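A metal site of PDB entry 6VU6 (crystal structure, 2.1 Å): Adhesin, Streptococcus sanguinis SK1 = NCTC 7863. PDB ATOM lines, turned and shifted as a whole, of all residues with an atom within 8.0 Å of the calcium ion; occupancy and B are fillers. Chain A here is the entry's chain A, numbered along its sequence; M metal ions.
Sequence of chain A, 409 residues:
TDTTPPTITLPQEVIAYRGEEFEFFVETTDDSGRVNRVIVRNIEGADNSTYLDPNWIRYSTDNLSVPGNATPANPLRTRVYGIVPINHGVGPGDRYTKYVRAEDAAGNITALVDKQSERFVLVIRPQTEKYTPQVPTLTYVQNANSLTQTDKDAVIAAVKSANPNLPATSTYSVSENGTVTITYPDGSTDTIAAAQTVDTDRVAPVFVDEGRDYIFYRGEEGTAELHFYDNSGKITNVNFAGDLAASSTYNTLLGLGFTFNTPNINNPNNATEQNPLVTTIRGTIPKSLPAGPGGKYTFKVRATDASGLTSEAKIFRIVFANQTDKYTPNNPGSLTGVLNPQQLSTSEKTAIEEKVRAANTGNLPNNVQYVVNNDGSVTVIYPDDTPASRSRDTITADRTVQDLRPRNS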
ATOM      1  N   TYR A 140       3.426  -5.159   9.196  1.00  0.00           N
ATOM      2  CA  TYR A 140       4.618  -4.619   9.867  1.00  0.00           C
ATOM      3  C   TYR A 140       5.471  -5.744  10.406  1.00  0.00           C
ATOM      4  O   TYR A 140       4.980  -6.532  11.146  1.00  0.00           O
ATOM      5  CB  TYR A 140       4.217  -3.640  10.964  1.00  0.00           C
ATOM      6  CG  TYR A 140       3.799  -2.301  10.451  1.00  0.00           C
ATOM      7  CD1 TYR A 140       4.714  -1.347  10.071  1.00  0.00           C
ATOM      8  CD2 TYR A 140       2.471  -1.995  10.313  1.00  0.00           C
ATOM      9  CE1 TYR A 140       4.309  -0.124   9.578  1.00  0.00           C
ATOM     10  CE2 TYR A 140       2.042  -0.787   9.821  1.00  0.00           C
ATOM     11  CZ  TYR A 140       2.971   0.161   9.467  1.00  0.00           C
ATOM     12  OH  TYR A 140       2.497   1.322   8.995  1.00  0.00           O
ATOM     13  N   VAL A 141       6.737  -5.790  10.028  1.00  0.00           N
ATOM     14  CA  VAL A 141       7.638  -6.896  10.461  1.00  0.00           C
ATOM     15  C   VAL A 141       8.889  -6.421  11.184  1.00  0.00           C
ATOM     16  O   VAL A 141       9.232  -5.274  11.109  1.00  0.00           O
ATOM     17  CB  VAL A 141       8.020  -7.769   9.270  1.00  0.00           C
ATOM     18  CG1 VAL A 141       6.808  -8.217   8.490  1.00  0.00           C
ATOM     19  CG2 VAL A 141       8.997  -7.033   8.365  1.00  0.00           C
ATOM     20  N   THR A 200       9.236  -2.363   7.929  1.00  0.00           N
ATOM     21  CA  THR A 200       9.896  -2.737   9.174  1.00  0.00           C
ATOM     22  C   THR A 200       9.161  -2.037  10.295  1.00  0.00           C
ATOM     23  O   THR A 200       8.921  -0.865  10.283  1.00  0.00           O
ATOM     24  CB  THR A 200      11.405  -2.553   9.129  1.00  0.00           C
ATOM     25  OG1 THR A 200      11.789  -2.461  10.491  1.00  0.00           O
ATOM     26  CG2 THR A 200      11.801  -1.322   8.381  1.00  0.00           C
ATOM     27  N   ASP A 201       8.819  -2.863  11.221  1.00  0.00           N
ATOM     28  CA  ASP A 201       8.094  -2.382  12.377  1.00  0.00           C
ATOM     29  C   ASP A 201       9.012  -1.522  13.258  1.00  0.00           C
ATOM     30  O   ASP A 201       9.809  -2.066  13.920  1.00  0.00           O
ATOM     31  CB  ASP A 201       7.600  -3.588  13.122  1.00  0.00           C
ATOM     32  CG  ASP A 201       6.545  -3.064  14.019  1.00  0.00           C
ATOM     33  OD1 ASP A 201       6.602  -1.868  14.386  1.00  0.00           O
ATOM     34  OD2 ASP A 201       5.600  -3.775  14.428  1.00  0.00           O
ATOM     35  N   ARG A 202       8.803  -0.221  13.270  1.00  0.00           N
ATOM     36  CA  ARG A 202       9.756   0.700  13.955  1.00  0.00           C
ATOM     37  C   ARG A 202       9.159   1.399  15.162  1.00  0.00           C
ATOM     38  O   ARG A 202       9.871   2.087  15.825  1.00  0.00           O
ATOM     39  CB  ARG A 202       9.987   1.855  12.984  1.00  0.00           C
ATOM     40  CG  ARG A 202      11.386   1.984  12.449  1.00  0.00           C
ATOM     41  CD  ARG A 202      11.262   3.364  11.870  1.00  0.00           C
ATOM     42  NE  ARG A 202      10.557   3.172  10.642  1.00  0.00           N
ATOM     43  CZ  ARG A 202       9.822   4.054  10.012  1.00  0.00           C
ATOM     44  NH1 ARG A 202       9.627   5.254  10.521  1.00  0.00           N
ATOM     45  NH2 ARG A 202       9.234   3.694   8.903  1.00  0.00           N
ATOM     46  N   VAL A 203       7.856   1.336  15.325  1.00  0.00           N
ATOM     47  CA  VAL A 203       7.260   2.092  16.438  1.00  0.00           C
ATOM     48  C   VAL A 203       6.551   1.150  17.401  1.00  0.00           C
ATOM     49  O   VAL A 203       5.624   0.588  17.067  1.00  0.00           O
ATOM     50  CB  VAL A 203       6.273   3.108  15.884  1.00  0.00           C
ATOM     51  CG1 VAL A 203       5.814   4.071  16.946  1.00  0.00           C
ATOM     52  CG2 VAL A 203       6.833   3.822  14.677  1.00  0.00           C
ATOM     53  N   ALA A 204       6.992   1.193  18.650  1.00  0.00           N
ATOM     54  CA  ALA A 204       6.398   0.418  19.766  1.00  0.00           C
ATOM     55  C   ALA A 204       4.949   0.843  20.092  1.00  0.00           C
ATOM     56  O   ALA A 204       4.500   1.916  19.708  1.00  0.00           O
ATOM     57  CB  ALA A 204       7.295   0.535  20.954  1.00  0.00           C
ATOM     58  N   PRO A 205       4.192  -0.001  20.801  1.00  0.00           N
ATOM     59  CA  PRO A 205       2.833   0.324  21.196  1.00  0.00           C
ATOM     60  C   PRO A 205       2.707   1.569  22.096  1.00  0.00           C
ATOM     61  O   PRO A 205       3.532   1.858  22.828  1.00  0.00           O
ATOM     62  CB  PRO A 205       2.343  -0.918  21.933  1.00  0.00           C
ATOM     63  CG  PRO A 205       3.245  -1.972  21.429  1.00  0.00           C
ATOM     64  CD  PRO A 205       4.573  -1.285  21.247  1.00  0.00           C
ATOM     65  N   VAL A 206       1.628   2.274  21.859  1.00  0.00           N
ATOM     66  CA  VAL A 206       1.240   3.511  22.571  1.00  0.00           C
ATOM     67  C   VAL A 206       0.235   3.180  23.684  1.00  0.00           C
ATOM     68  O   VAL A 206      -0.744   2.490  23.419  1.00  0.00           O
ATOM     69  CB  VAL A 206       0.652   4.543  21.602  1.00  0.00           C
ATOM     70  CG1 VAL A 206       0.060   5.719  22.325  1.00  0.00           C
ATOM     71  CG2 VAL A 206       1.627   4.981  20.533  1.00  0.00           C
ATOM     72  N   TYR A 229      -2.872   0.900  21.683  1.00  0.00           N
ATOM     73  CA  TYR A 229      -2.946   0.461  20.306  1.00  0.00           C
ATOM     74  C   TYR A 229      -1.530   0.316  19.771  1.00  0.00           C
ATOM     75  O   TYR A 229      -0.548   0.537  20.487  1.00  0.00           O
ATOM     76  CB  TYR A 229      -3.797   1.417  19.462  1.00  0.00           C
ATOM     77  CG  TYR A 229      -3.235   2.803  19.371  1.00  0.00           C
ATOM     78  CD1 TYR A 229      -2.312   3.129  18.385  1.00  0.00           C
ATOM     79  CD2 TYR A 229      -3.613   3.781  20.270  1.00  0.00           C
ATOM     80  CE1 TYR A 229      -1.787   4.386  18.301  1.00  0.00           C
ATOM     81  CE2 TYR A 229      -3.097   5.052  20.190  1.00  0.00           C
ATOM     82  CZ  TYR A 229      -2.180   5.348  19.203  1.00  0.00           C
ATOM     83  OH  TYR A 229      -1.651   6.624  19.113  1.00  0.00           O
ATOM     84  N   ASP A 230      -1.422  -0.073  18.511  1.00  0.00           N
ATOM     85  CA  ASP A 230      -0.123  -0.158  17.853  1.00  0.00           C
ATOM     86  C   ASP A 230      -0.314   0.243  16.404  1.00  0.00           C
ATOM     87  O   ASP A 230      -1.424   0.154  15.869  1.00  0.00           O
ATOM     88  CB  ASP A 230       0.499  -1.569  17.953  1.00  0.00           C
ATOM     89  CG  ASP A 230       1.964  -1.613  17.476  1.00  0.00           C
ATOM     90  OD1 ASP A 230       2.853  -0.974  18.098  1.00  0.00           O
ATOM     91  OD2 ASP A 230       2.243  -2.314  16.478  1.00  0.00           O
ATOM     92  N   ASN A 231       0.779   0.664  15.775  1.00  0.00           N
ATOM     93  CA  ASN A 231       0.721   0.971  14.346  1.00  0.00           C
ATOM     94  C   ASN A 231       0.395  -0.285  13.542  1.00  0.00           C
ATOM     95  O   ASN A 231      -0.354  -0.218  12.560  1.00  0.00           O
ATOM     96  CB  ASN A 231       2.039   1.594  13.874  1.00  0.00           C
ATOM     97  CG  ASN A 231       3.249   0.712  14.107  1.00  0.00           C
ATOM     98  OD1 ASN A 231       3.292  -0.106  15.046  1.00  0.00           O
ATOM     99  ND2 ASN A 231       4.252   0.879  13.274  1.00  0.00           N
ATOM    100  N   SER A 232       0.898  -1.442  13.984  1.00  0.00           N
ATOM    101  CA  SER A 232       0.526  -2.714  13.371  1.00  0.00           C
ATOM    102  C   SER A 232      -0.899  -3.106  13.693  1.00  0.00           C
ATOM    103  O   SER A 232      -1.437  -3.999  13.042  1.00  0.00           O
ATOM    104  CB  SER A 232       1.460  -3.830  13.834  1.00  0.00           C
ATOM    105  OG  SER A 232       1.105  -4.258  15.134  1.00  0.00           O
ATOM    106  N   GLY A 233      -1.515  -2.504  14.706  1.00  0.00           N
ATOM    107  CA  GLY A 233      -2.815  -2.942  15.128  1.00  0.00           C
ATOM    108  C   GLY A 233      -2.853  -4.273  15.868  1.00  0.00           C
ATOM    109  O   GLY A 233      -3.949  -4.809  16.076  1.00  0.00           O
ATOM    110  N   LYS A 234      -1.705  -4.804  16.279  1.00  0.00           N
ATOM    111  CA  LYS A 234      -1.640  -6.076  16.983  1.00  0.00           C
ATOM    112  C   LYS A 234      -0.696  -5.982  18.175  1.00  0.00           C
ATOM    113  O   LYS A 234       0.477  -5.623  18.018  1.00  0.00           O
ATOM    114  CB  LYS A 234      -1.163  -7.205  16.066  1.00  0.00           C
ATOM    115  CG  LYS A 234      -0.794  -8.468  16.824  1.00  0.00           C
ATOM    116  CD  LYS A 234      -1.992  -9.087  17.559  1.00  0.00           C
ATOM    117  CE  LYS A 234      -1.567 -10.299  18.393  1.00  0.00           C
ATOM    118  NZ  LYS A 234      -2.669 -10.949  19.184  1.00  0.00           N
ATOM    119  N   ILE A 235      -1.206  -6.330  19.349  1.00  0.00           N
ATOM    120  CA  ILE A 235      -0.400  -6.374  20.567  1.00  0.00           C
ATOM    121  C   ILE A 235      -0.444  -7.794  21.112  1.00  0.00           C
ATOM    122  O   ILE A 235      -1.511  -8.414  21.215  1.00  0.00           O
ATOM    123  CB  ILE A 235      -0.883  -5.347  21.604  1.00  0.00           C
ATOM    124  CG1 ILE A 235      -0.460  -3.956  21.158  1.00  0.00           C
ATOM    125  CG2 ILE A 235      -0.311  -5.631  22.996  1.00  0.00           C
ATOM    126  CD1 ILE A 235      -1.038  -2.859  21.986  1.00  0.00           C
ATOM    127  N   THR A 304       4.184  -5.070  24.049  1.00  0.00           N
ATOM    128  CA  THR A 304       4.983  -5.560  22.929  1.00  0.00           C
ATOM    129  C   THR A 304       4.101  -5.947  21.752  1.00  0.00           C
ATOM    130  O   THR A 304       3.002  -6.479  21.937  1.00  0.00           O
ATOM    131  CB  THR A 304       5.829  -6.764  23.377  1.00  0.00           C
ATOM    132  OG1 THR A 304       6.606  -6.398  24.534  1.00  0.00           O
ATOM    133  CG2 THR A 304       6.784  -7.224  22.281  1.00  0.00           C
ATOM    134  N   ASP A 305       4.561  -5.642  20.531  1.00  0.00           N
ATOM    135  CA  ASP A 305       3.832  -6.023  19.332  1.00  0.00           C
ATOM    136  C   ASP A 305       4.403  -7.330  18.768  1.00  0.00           C
ATOM    137  O   ASP A 305       5.298  -7.933  19.359  1.00  0.00           O
ATOM    138  CB  ASP A 305       3.831  -4.873  18.317  1.00  0.00           C
ATOM    139  CG  ASP A 305       5.229  -4.462  17.856  1.00  0.00           C
ATOM    140  OD1 ASP A 305       6.170  -5.297  17.935  1.00  0.00           O
ATOM    141  OD2 ASP A 305       5.384  -3.301  17.374  1.00  0.00           O
ATOM    142  N   ALA A 306       3.881  -7.776  17.613  1.00  0.00           N
ATOM    143  CA  ALA A 306       4.295  -9.068  17.063  1.00  0.00           C
ATOM    144  C   ALA A 306       5.725  -9.029  16.542  1.00  0.00           C
ATOM    145  O   ALA A 306       6.370 -10.085  16.481  1.00  0.00           O
ATOM    146  CB  ALA A 306       3.342  -9.522  15.961  1.00  0.00           C
ATOM    147  N   SER A 307       6.240  -7.865  16.178  1.00  0.00           N
ATOM    148  CA  SER A 307       7.639  -7.721  15.798  1.00  0.00           C
ATOM    149  C   SER A 307       8.589  -7.705  16.985  1.00  0.00           C
ATOM    150  O   SER A 307       9.771  -7.376  16.808  1.00  0.00           O
ATOM    151  CB  SER A 307       7.845  -6.441  15.005  1.00  0.00           C
ATOM    152  OG  SER A 307       8.062  -5.366  15.898  1.00  0.00           O
ATOM    153  N   GLY A 308       8.105  -7.998  18.187  1.00  0.00           N
ATOM    154  CA  GLY A 308       8.951  -7.936  19.364  1.00  0.00           C
ATOM    155  C   GLY A 308       9.390  -6.556  19.823  1.00  0.00           C
ATOM    156  O   GLY A 308      10.220  -6.463  20.730  1.00  0.00           O
ATOM    157  N   LEU A 309       8.874  -5.473  19.232  1.00  0.00           N
ATOM    158  CA  LEU A 309       9.197  -4.143  19.744  1.00  0.00           C
ATOM    159  C   LEU A 309       8.420  -3.879  21.030  1.00  0.00           C
ATOM    160  O   LEU A 309       7.211  -4.105  21.093  1.00  0.00           O
ATOM    161  CB  LEU A 309       8.850  -3.079  18.705  1.00  0.00           C
ATOM    162  CG  LEU A 309       9.913  -2.092  18.208  1.00  0.00           C
ATOM    163  CD1 LEU A 309       9.252  -0.814  17.742  1.00  0.00           C
ATOM    164  CD2 LEU A 309      10.988  -1.803  19.268  1.00  0.00           C
ATOM    165  N   THR A 310       9.175  -3.731  22.088  1.00  0.00           N
ATOM    166  CA  THR A 310       8.539  -3.478  23.389  1.00  0.00           C
ATOM    167  C   THR A 310       8.617  -1.986  23.647  1.00  0.00           C
ATOM    168  O   THR A 310       9.610  -1.429  23.308  1.00  0.00           O
ATOM    169  CB  THR A 310       9.240  -4.275  24.486  1.00  0.00           C
ATOM    170  OG1 THR A 310       9.063  -5.649  24.173  1.00  0.00           O
ATOM    171  CG2 THR A 310       8.651  -3.985  25.846  1.00  0.00           C
HETATM  172 CA    CA M   1       4.700  -1.724  16.161  1.00  0.00          CA
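The calcium ion is bound by OD2 of Asp 305, at 2.1 Å.
OD1 of Asn 231 binds the calcium ion (2.4 Å).
The calcium ion is bound by the side-chain carboxylate (OD2) of Asp 230.
OD1 of Asp 201 is bound to the calcium ion (2.6 Å).
O of Val 203 binds the calcium ion, 2.6 Å away.
The calcium ion is bound by OD1 of Asp 230, at 2.8 Å.
The side-chain carboxylate (OD2) of Asp 201 binds the calcium ion (2.8 Å).
N of Leu 309 lies within hydrogen-bond range of OD1 of Asp 305 (3.0 Å).
The side-chain hydroxyl (OG) of Ser 307 sits close to the side-chain carboxylate (OD2) of Asp 201, at 3.3 Å.
The side-chain carboxylate of Asp 230 lies close to the side-chain hydroxyl of Ser 232 (2.6 Å).
The backbone NH (N) of Asp 201 is in hydrogen-bond range of the backbone carbonyl oxygen (O) of Val 141 (2.4 Å).
The side-chain carboxylate (OD1) of Asp 305 is in hydrogen-bond range of the backbone NH (N) of Gly 308 (3.3 Å).
The side-chain carboxylate (OD1) of Asp 305 lies within hydrogen-bond range of the side-chain hydroxyl (OG) of Ser 307, at 2.8 Å.
Of the 23 residues printed, 5 come within 4 Å of the calcium ion.
Along chain A the residues within 4 Å of the calcium ion span positions 201 to 305.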
